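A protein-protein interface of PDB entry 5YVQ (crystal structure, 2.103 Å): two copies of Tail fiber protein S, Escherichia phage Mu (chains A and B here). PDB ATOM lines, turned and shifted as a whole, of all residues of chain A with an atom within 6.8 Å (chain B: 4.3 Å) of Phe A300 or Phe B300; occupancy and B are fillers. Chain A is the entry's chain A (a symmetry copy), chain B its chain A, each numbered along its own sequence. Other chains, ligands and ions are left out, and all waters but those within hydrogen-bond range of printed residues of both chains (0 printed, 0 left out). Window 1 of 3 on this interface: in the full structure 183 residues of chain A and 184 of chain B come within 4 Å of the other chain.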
ATOM      1  N   PHE A 289     -27.484 -24.765   4.977  1.00  0.00           N
ATOM      2  CA  PHE A 289     -27.066 -23.380   5.129  1.00  0.00           C
ATOM      3  C   PHE A 289     -28.291 -22.525   5.423  1.00  0.00           C
ATOM      4  O   PHE A 289     -29.312 -22.642   4.732  1.00  0.00           O
ATOM      5  CB  PHE A 289     -26.362 -22.871   3.855  1.00  0.00           C
ATOM      6  CG  PHE A 289     -26.295 -21.362   3.772  1.00  0.00           C
ATOM      7  CD1 PHE A 289     -25.295 -20.660   4.433  1.00  0.00           C
ATOM      8  CD2 PHE A 289     -27.239 -20.646   3.052  1.00  0.00           C
ATOM      9  CE1 PHE A 289     -25.244 -19.267   4.368  1.00  0.00           C
ATOM     10  CE2 PHE A 289     -27.185 -19.259   2.987  1.00  0.00           C
ATOM     11  CZ  PHE A 289     -26.186 -18.569   3.640  1.00  0.00           C
ATOM     12  N   PHE A 290     -28.199 -21.641   6.411  1.00  0.00           N
ATOM     13  CA  PHE A 290     -29.315 -20.719   6.567  1.00  0.00           C
ATOM     14  C   PHE A 290     -28.858 -19.379   7.093  1.00  0.00           C
ATOM     15  O   PHE A 290     -27.792 -19.245   7.703  1.00  0.00           O
ATOM     16  CB  PHE A 290     -30.446 -21.275   7.448  1.00  0.00           C
ATOM     17  CG  PHE A 290     -30.062 -21.687   8.832  1.00  0.00           C
ATOM     18  CD1 PHE A 290     -29.488 -22.931   9.076  1.00  0.00           C
ATOM     19  CD2 PHE A 290     -30.394 -20.881   9.925  1.00  0.00           C
ATOM     20  CE1 PHE A 290     -29.181 -23.335  10.382  1.00  0.00           C
ATOM     21  CE2 PHE A 290     -30.092 -21.294  11.234  1.00  0.00           C
ATOM     22  CZ  PHE A 290     -29.492 -22.523  11.451  1.00  0.00           C
ATOM     23  N   ILE A 291     -29.693 -18.382   6.831  1.00  0.00           N
ATOM     24  CA  ILE A 291     -29.491 -17.027   7.331  1.00  0.00           C
ATOM     25  C   ILE A 291     -30.407 -16.848   8.527  1.00  0.00           C
ATOM     26  O   ILE A 291     -31.617 -17.089   8.437  1.00  0.00           O
ATOM     27  CB  ILE A 291     -29.769 -15.983   6.240  1.00  0.00           C
ATOM     28  CG1 ILE A 291     -28.859 -16.255   5.035  1.00  0.00           C
ATOM     29  CG2 ILE A 291     -29.624 -14.544   6.786  1.00  0.00           C
ATOM     30  CD1 ILE A 291     -29.099 -15.341   3.846  1.00  0.00           C
ATOM     31  N   ARG A 292     -29.834 -16.479   9.664  1.00  0.00           N
ATOM     32  CA  ARG A 292     -30.598 -16.246  10.877  1.00  0.00           C
ATOM     33  C   ARG A 292     -30.463 -14.787  11.273  1.00  0.00           C
ATOM     34  O   ARG A 292     -29.349 -14.315  11.557  1.00  0.00           O
ATOM     35  CB  ARG A 292     -30.124 -17.161  12.007  1.00  0.00           C
ATOM     36  CG  ARG A 292     -30.704 -16.783  13.364  1.00  0.00           C
ATOM     37  CD  ARG A 292     -30.171 -17.718  14.446  1.00  0.00           C
ATOM     38  NE  ARG A 292     -30.634 -17.320  15.765  1.00  0.00           N
ATOM     39  CZ  ARG A 292     -31.757 -17.765  16.318  1.00  0.00           C
ATOM     40  NH1 ARG A 292     -32.533 -18.619  15.663  1.00  0.00           N
ATOM     41  NH2 ARG A 292     -32.103 -17.350  17.517  1.00  0.00           N
ATOM     42  N   THR A 298     -27.412 -10.566  12.241  1.00  0.00           N
ATOM     43  CA  THR A 298     -27.750 -11.479  11.152  1.00  0.00           C
ATOM     44  C   THR A 298     -26.566 -12.412  10.922  1.00  0.00           C
ATOM     45  O   THR A 298     -25.449 -11.945  10.663  1.00  0.00           O
ATOM     46  CB  THR A 298     -28.074 -10.700   9.872  1.00  0.00           C
ATOM     47  OG1 THR A 298     -29.185  -9.829  10.111  1.00  0.00           O
ATOM     48  CG2 THR A 298     -28.400 -11.643   8.721  1.00  0.00           C
ATOM     49  N   TYR A 299     -26.805 -13.718  11.037  1.00  0.00           N
ATOM     50  CA  TYR A 299     -25.763 -14.731  10.938  1.00  0.00           C
ATOM     51  C   TYR A 299     -25.897 -15.537   9.652  1.00  0.00           C
ATOM     52  O   TYR A 299     -27.015 -15.850   9.207  1.00  0.00           O
ATOM     53  CB  TYR A 299     -25.808 -15.703  12.131  1.00  0.00           C
ATOM     54  CG  TYR A 299     -25.600 -15.049  13.490  1.00  0.00           C
ATOM     55  CD1 TYR A 299     -26.673 -14.479  14.183  1.00  0.00           C
ATOM     56  CD2 TYR A 299     -24.343 -15.023  14.094  1.00  0.00           C
ATOM     57  CE1 TYR A 299     -26.507 -13.881  15.433  1.00  0.00           C
ATOM     58  CE2 TYR A 299     -24.153 -14.403  15.368  1.00  0.00           C
ATOM     59  CZ  TYR A 299     -25.245 -13.841  16.023  1.00  0.00           C
ATOM     60  OH  TYR A 299     -25.115 -13.242  17.265  1.00  0.00           O
ATOM     61  N   PHE A 300     -24.760 -15.913   9.085  1.00  0.00           N
ATOM     62  CA  PHE A 300     -24.711 -17.010   8.115  1.00  0.00           C
ATOM     63  C   PHE A 300     -24.423 -18.302   8.869  1.00  0.00           C
ATOM     64  O   PHE A 300     -23.335 -18.471   9.440  1.00  0.00           O
ATOM     65  CB  PHE A 300     -23.669 -16.760   7.033  1.00  0.00           C
ATOM     66  CG  PHE A 300     -23.997 -15.604   6.136  1.00  0.00           C
ATOM     67  CD1 PHE A 300     -25.123 -14.831   6.356  1.00  0.00           C
ATOM     68  CD2 PHE A 300     -23.187 -15.296   5.065  1.00  0.00           C
ATOM     69  CE1 PHE A 300     -25.434 -13.765   5.531  1.00  0.00           C
ATOM     70  CE2 PHE A 300     -23.488 -14.229   4.241  1.00  0.00           C
ATOM     71  CZ  PHE A 300     -24.626 -13.470   4.474  1.00  0.00           C
ATOM     72  N   MET A 301     -25.398 -19.216   8.888  1.00  0.00           N
ATOM     73  CA  MET A 301     -25.345 -20.373   9.770  1.00  0.00           C
ATOM     74  C   MET A 301     -25.216 -21.673   8.986  1.00  0.00           C
ATOM     75  O   MET A 301     -25.640 -21.783   7.830  1.00  0.00           O
ATOM     76  CB  MET A 301     -26.588 -20.443  10.672  1.00  0.00           C
ATOM     77  CG  MET A 301     -26.708 -19.309  11.726  1.00  0.00           C
ATOM     78  SD  MET A 301     -25.287 -19.238  12.855  1.00  0.00           S
ATOM     79  CE  MET A 301     -26.040 -18.621  14.361  1.00  0.00           C
ATOM     80  N   LEU A 302     -24.677 -22.681   9.679  1.00  0.00           N
ATOM     81  CA  LEU A 302     -24.434 -24.021   9.158  1.00  0.00           C
ATOM     82  C   LEU A 302     -24.950 -25.048  10.154  1.00  0.00           C
ATOM     83  O   LEU A 302     -24.849 -24.853  11.369  1.00  0.00           O
ATOM     84  CB  LEU A 302     -22.922 -24.268   8.911  1.00  0.00           C
ATOM     85  CG  LEU A 302     -22.246 -23.412   7.835  1.00  0.00           C
ATOM     86  CD1 LEU A 302     -20.683 -23.481   7.901  1.00  0.00           C
ATOM     87  CD2 LEU A 302     -22.751 -23.786   6.446  1.00  0.00           C
ATOM     88  N   LEU A 315     -20.218 -23.081  14.490  1.00  0.00           N
ATOM     89  CA  LEU A 315     -19.549 -22.271  13.476  1.00  0.00           C
ATOM     90  C   LEU A 315     -20.208 -20.897  13.314  1.00  0.00           C
ATOM     91  O   LEU A 315     -21.439 -20.781  13.234  1.00  0.00           O
ATOM     92  CB  LEU A 315     -19.564 -23.013  12.131  1.00  0.00           C
ATOM     93  CG  LEU A 315     -18.832 -24.351  12.148  1.00  0.00           C
ATOM     94  CD1 LEU A 315     -18.822 -25.011  10.779  1.00  0.00           C
ATOM     95  CD2 LEU A 315     -17.392 -24.129  12.669  1.00  0.00           C
ATOM     96  N   ARG A 316     -19.377 -19.850  13.215  1.00  0.00           N
ATOM     97  CA  ARG A 316     -19.826 -18.505  12.845  1.00  0.00           C
ATOM     98  C   ARG A 316     -18.994 -17.996  11.670  1.00  0.00           C
ATOM     99  O   ARG A 316     -18.103 -17.149  11.836  1.00  0.00           O
ATOM    100  CB  ARG A 316     -19.753 -17.544  14.041  1.00  0.00           C
ATOM    101  CG  ARG A 316     -20.467 -18.032  15.299  1.00  0.00           C
ATOM    102  CD  ARG A 316     -22.000 -18.032  15.086  1.00  0.00           C
ATOM    103  NE  ARG A 316     -22.713 -18.407  16.307  1.00  0.00           N
ATOM    104  CZ  ARG A 316     -23.163 -19.628  16.569  1.00  0.00           C
ATOM    105  NH1 ARG A 316     -22.999 -20.605  15.685  1.00  0.00           N
ATOM    106  NH2 ARG A 316     -23.783 -19.867  17.717  1.00  0.00           N
ATOM    107  N   PRO A 317     -19.248 -18.504  10.458  1.00  0.00           N
ATOM    108  CA  PRO A 317     -18.477 -18.019   9.291  1.00  0.00           C
ATOM    109  C   PRO A 317     -18.567 -16.518   9.063  1.00  0.00           C
ATOM    110  O   PRO A 317     -17.547 -15.877   8.749  1.00  0.00           O
ATOM    111  CB  PRO A 317     -19.062 -18.814   8.117  1.00  0.00           C
ATOM    112  CG  PRO A 317     -20.354 -19.442   8.639  1.00  0.00           C
ATOM    113  CD  PRO A 317     -20.161 -19.610  10.115  1.00  0.00           C
ATOM    114  N   LEU A 318     -19.741 -15.928   9.242  1.00  0.00           N
ATOM    115  CA  LEU A 318     -19.923 -14.514   8.963  1.00  0.00           C
ATOM    116  C   LEU A 318     -21.179 -14.028   9.657  1.00  0.00           C
ATOM    117  O   LEU A 318     -22.214 -14.702   9.597  1.00  0.00           O
ATOM    118  CB  LEU A 318     -20.038 -14.267   7.448  1.00  0.00           C
ATOM    119  CG  LEU A 318     -19.958 -12.792   7.042  1.00  0.00           C
ATOM    120  CD1 LEU A 318     -19.359 -12.675   5.679  1.00  0.00           C
ATOM    121  CD2 LEU A 318     -21.304 -12.125   7.070  1.00  0.00           C
ATOM    122  N   TRP A 319     -21.108 -12.840  10.263  1.00  0.00           N
ATOM    123  CA  TRP A 319     -22.316 -12.197  10.757  1.00  0.00           C
ATOM    124  C   TRP A 319     -22.222 -10.682  10.642  1.00  0.00           C
ATOM    125  O   TRP A 319     -21.142 -10.101  10.458  1.00  0.00           O
ATOM    126  CB  TRP A 319     -22.644 -12.627  12.194  1.00  0.00           C
ATOM    127  CG  TRP A 319     -21.762 -12.159  13.295  1.00  0.00           C
ATOM    128  CD1 TRP A 319     -21.984 -11.089  14.115  1.00  0.00           C
ATOM    129  CD2 TRP A 319     -20.552 -12.775  13.758  1.00  0.00           C
ATOM    130  NE1 TRP A 319     -20.987 -10.986  15.034  1.00  0.00           N
ATOM    131  CE2 TRP A 319     -20.086 -11.999  14.843  1.00  0.00           C
ATOM    132  CE3 TRP A 319     -19.809 -13.896  13.353  1.00  0.00           C
ATOM    133  CZ2 TRP A 319     -18.892 -12.307  15.547  1.00  0.00           C
ATOM    134  CZ3 TRP A 319     -18.615 -14.202  14.054  1.00  0.00           C
ATOM    135  CH2 TRP A 319     -18.175 -13.406  15.135  1.00  0.00           C
ATOM    136  N   ILE A 320     -23.385 -10.047  10.736  1.00  0.00           N
ATOM    137  CA  ILE A 320     -23.515  -8.601  10.618  1.00  0.00           C
ATOM    138  C   ILE A 320     -24.186  -8.062  11.872  1.00  0.00           C
ATOM    139  O   ILE A 320     -25.185  -8.616  12.341  1.00  0.00           O
ATOM    140  CB  ILE A 320     -24.311  -8.204   9.362  1.00  0.00           C
ATOM    141  CG1 ILE A 320     -23.622  -8.747   8.111  1.00  0.00           C
ATOM    142  CG2 ILE A 320     -24.528  -6.698   9.315  1.00  0.00           C
ATOM    143  CD1 ILE A 320     -24.476  -8.616   6.840  1.00  0.00           C
ATOM    144  N   PHE B 289     -33.430  -7.535   7.931  1.00  0.00           N
ATOM    145  CA  PHE B 289     -32.303  -7.801   7.050  1.00  0.00           C
ATOM    146  C   PHE B 289     -32.832  -8.179   5.673  1.00  0.00           C
ATOM    147  O   PHE B 289     -33.734  -9.021   5.562  1.00  0.00           O
ATOM    148  CB  PHE B 289     -31.423  -8.940   7.607  1.00  0.00           C
ATOM    149  CG  PHE B 289     -30.513  -9.555   6.566  1.00  0.00           C
ATOM    150  CD1 PHE B 289     -29.297  -8.961   6.250  1.00  0.00           C
ATOM    151  CD2 PHE B 289     -30.880 -10.709   5.893  1.00  0.00           C
ATOM    152  CE1 PHE B 289     -28.466  -9.520   5.279  1.00  0.00           C
ATOM    153  CE2 PHE B 289     -30.050 -11.266   4.928  1.00  0.00           C
ATOM    154  CZ  PHE B 289     -28.842 -10.676   4.624  1.00  0.00           C
ATOM    155  N   PHE B 290     -32.264  -7.602   4.619  1.00  0.00           N
ATOM    156  CA  PHE B 290     -32.663  -8.098   3.310  1.00  0.00           C
ATOM    157  C   PHE B 290     -31.534  -8.006   2.313  1.00  0.00           C
ATOM    158  O   PHE B 290     -30.584  -7.231   2.471  1.00  0.00           O
ATOM    159  CB  PHE B 290     -33.919  -7.406   2.753  1.00  0.00           C
ATOM    160  CG  PHE B 290     -33.848  -5.919   2.620  1.00  0.00           C
ATOM    161  CD1 PHE B 290     -34.081  -5.091   3.713  1.00  0.00           C
ATOM    162  CD2 PHE B 290     -33.675  -5.332   1.364  1.00  0.00           C
ATOM    163  CE1 PHE B 290     -34.069  -3.697   3.572  1.00  0.00           C
ATOM    164  CE2 PHE B 290     -33.672  -3.933   1.224  1.00  0.00           C
ATOM    165  CZ  PHE B 290     -33.874  -3.127   2.331  1.00  0.00           C
ATOM    166  N   ILE B 291     -31.655  -8.827   1.279  1.00  0.00           N
ATOM    167  CA  ILE B 291     -30.726  -8.830   0.155  1.00  0.00           C
ATOM    168  C   ILE B 291     -31.391  -8.072  -0.979  1.00  0.00           C
ATOM    169  O   ILE B 291     -32.523  -8.383  -1.367  1.00  0.00           O
ATOM    170  CB  ILE B 291     -30.355 -10.262  -0.257  1.00  0.00           C
ATOM    171  CG1 ILE B 291     -29.748 -10.994   0.947  1.00  0.00           C
ATOM    172  CG2 ILE B 291     -29.425 -10.271  -1.493  1.00  0.00           C
ATOM    173  CD1 ILE B 291     -29.417 -12.455   0.692  1.00  0.00           C
ATOM    174  N   TYR B 299     -26.672  -6.045  -2.621  1.00  0.00           N
ATOM    175  CA  TYR B 299     -26.385  -5.484  -1.307  1.00  0.00           C
ATOM    176  C   TYR B 299     -26.941  -6.367  -0.197  1.00  0.00           C
ATOM    177  O   TYR B 299     -28.035  -6.942  -0.323  1.00  0.00           O
ATOM    178  CB  TYR B 299     -26.983  -4.073  -1.156  1.00  0.00           C
ATOM    179  CG  TYR B 299     -26.454  -3.049  -2.151  1.00  0.00           C
ATOM    180  CD1 TYR B 299     -27.022  -2.926  -3.423  1.00  0.00           C
ATOM    181  CD2 TYR B 299     -25.408  -2.190  -1.815  1.00  0.00           C
ATOM    182  CE1 TYR B 299     -26.557  -1.990  -4.349  1.00  0.00           C
ATOM    183  CE2 TYR B 299     -24.912  -1.235  -2.755  1.00  0.00           C
ATOM    184  CZ  TYR B 299     -25.500  -1.146  -4.014  1.00  0.00           C
ATOM    185  OH  TYR B 299     -25.065  -0.227  -4.955  1.00  0.00           O
ATOM    186  N   PHE B 300     -26.211  -6.433   0.909  1.00  0.00           N
ATOM    187  CA  PHE B 300     -26.783  -6.877   2.181  1.00  0.00           C
ATOM    188  C   PHE B 300     -27.283  -5.652   2.934  1.00  0.00           C
ATOM    189  O   PHE B 300     -26.487  -4.794   3.345  1.00  0.00           O
ATOM    190  CB  PHE B 300     -25.773  -7.660   3.010  1.00  0.00           C
ATOM    191  CG  PHE B 300     -25.381  -8.972   2.402  1.00  0.00           C
ATOM    192  CD1 PHE B 300     -25.874  -9.359   1.169  1.00  0.00           C
ATOM    193  CD2 PHE B 300     -24.529  -9.827   3.067  1.00  0.00           C
ATOM    194  CE1 PHE B 300     -25.519 -10.571   0.602  1.00  0.00           C
ATOM    195  CE2 PHE B 300     -24.166 -11.035   2.505  1.00  0.00           C
ATOM    196  CZ  PHE B 300     -24.677 -11.408   1.271  1.00  0.00           C
ATOM    197  N   MET B 301     -28.605  -5.554   3.111  1.00  0.00           N
ATOM    198  CA  MET B 301     -29.224  -4.326   3.589  1.00  0.00           C
ATOM    199  C   MET B 301     -29.846  -4.509   4.967  1.00  0.00           C
ATOM    200  O   MET B 301     -30.248  -5.610   5.361  1.00  0.00           O
ATOM    201  CB  MET B 301     -30.296  -3.824   2.608  1.00  0.00           C
ATOM    202  CG  MET B 301     -29.762  -3.337   1.234  1.00  0.00           C
ATOM    203  SD  MET B 301     -28.561  -1.983   1.380  1.00  0.00           S
ATOM    204  CE  MET B 301     -28.846  -1.068  -0.135  1.00  0.00           C
ATOM    205  N   PRO B 317     -23.146  -2.797   4.953  1.00  0.00           N
ATOM    206  CA  PRO B 317     -22.225  -3.812   5.512  1.00  0.00           C
ATOM    207  C   PRO B 317     -21.448  -4.595   4.465  1.00  0.00           C
ATOM    208  O   PRO B 317     -20.242  -4.843   4.646  1.00  0.00           O
ATOM    209  CB  PRO B 317     -23.148  -4.718   6.338  1.00  0.00           C
ATOM    210  CG  PRO B 317     -24.573  -4.362   5.917  1.00  0.00           C
ATOM    211  CD  PRO B 317     -24.521  -2.934   5.466  1.00  0.00           C
ATOM    212  N   LEU B 318     -22.084  -4.963   3.361  1.00  0.00           N
ATOM    213  CA  LEU B 318     -21.431  -5.783   2.356  1.00  0.00           C
ATOM    214  C   LEU B 318     -22.198  -5.676   1.053  1.00  0.00           C
ATOM    215  O   LEU B 318     -23.432  -5.753   1.059  1.00  0.00           O
ATOM    216  CB  LEU B 318     -21.372  -7.254   2.804  1.00  0.00           C
ATOM    217  CG  LEU B 318     -20.468  -8.140   1.942  1.00  0.00           C
ATOM    218  CD1 LEU B 318     -19.895  -9.239   2.775  1.00  0.00           C
ATOM    219  CD2 LEU B 318     -21.200  -8.718   0.764  1.00  0.00           C
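Among the printed residues, pairs that only touch across the chains: Phe A300 with Phe B300 (3.2 Å), Thr A298 with Phe B289 (3.5 Å), Ile A291 with Phe B289 (3.8 Å), Ile A320 with Pro B317 (3.8 Å) and Ile A320 with Phe B300 (3.96 Å).
Phe B300 touches just these residues of chain A: Phe A300 (3.2 Å) and Ile A320 (3.96 Å). Printed residues of chain A within 4 Å of Pro B317: Ile A320 (3.8 Å). Printed residues of chain B within 4 Å of Thr A298: Phe B289 (3.5 Å). Printed residues of chain B within 4 Å of Ile A291: Phe B289. Printed residues of chain A within 4 Å of Phe B289: Ile A291 (3.8 Å) and Thr A298 (3.5 Å). Met B301 touches none of the printed residues of chain A. Leu A318 touches none of the printed residues of chain B. The nearest residue of chain A that does not touch Phe B300 is Leu A318 (5.5 Å).
N of Phe A300 lies within hydrogen-bond range of O of Leu A318 (2.9 Å). The backbone NH (N) of Phe B300 lies within hydrogen-bond range of the backbone carbonyl oxygen (O) of Leu B318, 2.9 Å away. The backbone carbonyl oxygen (O) of Thr A298 is in hydrogen-bond range of the backbone NH (N) of Ile A320, at 2.8 Å.
Ile A291 touches Phe B289, but with the chains exchanged Phe A289 does not touch Ile B291 (7.5 Å). Phe B300 touches its own counterpart, Phe A300. Positions printed for both chains: 289, 290, 291, 299, 300, 301, 317 and 318. Of the 5 pairs that touch across the chains among the printed residues, 1 has its exchanged pair printed and touching as well.
Of the 15 printed residues of chain A, 4 touch a printed residue of chain B. Printed residues of chain A that touch a printed residue of chain B: Ile A291, Thr A298, Phe A300 and Ile A320. Hydrophobic or aromatic side chains of chain B within 4 Å of the printed part of chain A: Phe B289, Phe B300 and Pro B317. Along chain B the printed residues that touch a printed residue of chain A span positions 289 to 317. Among the printed residues, no Asp or Glu carboxylate lies within 4 Å of a Lys or Arg side-chain nitrogen of the other chain.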
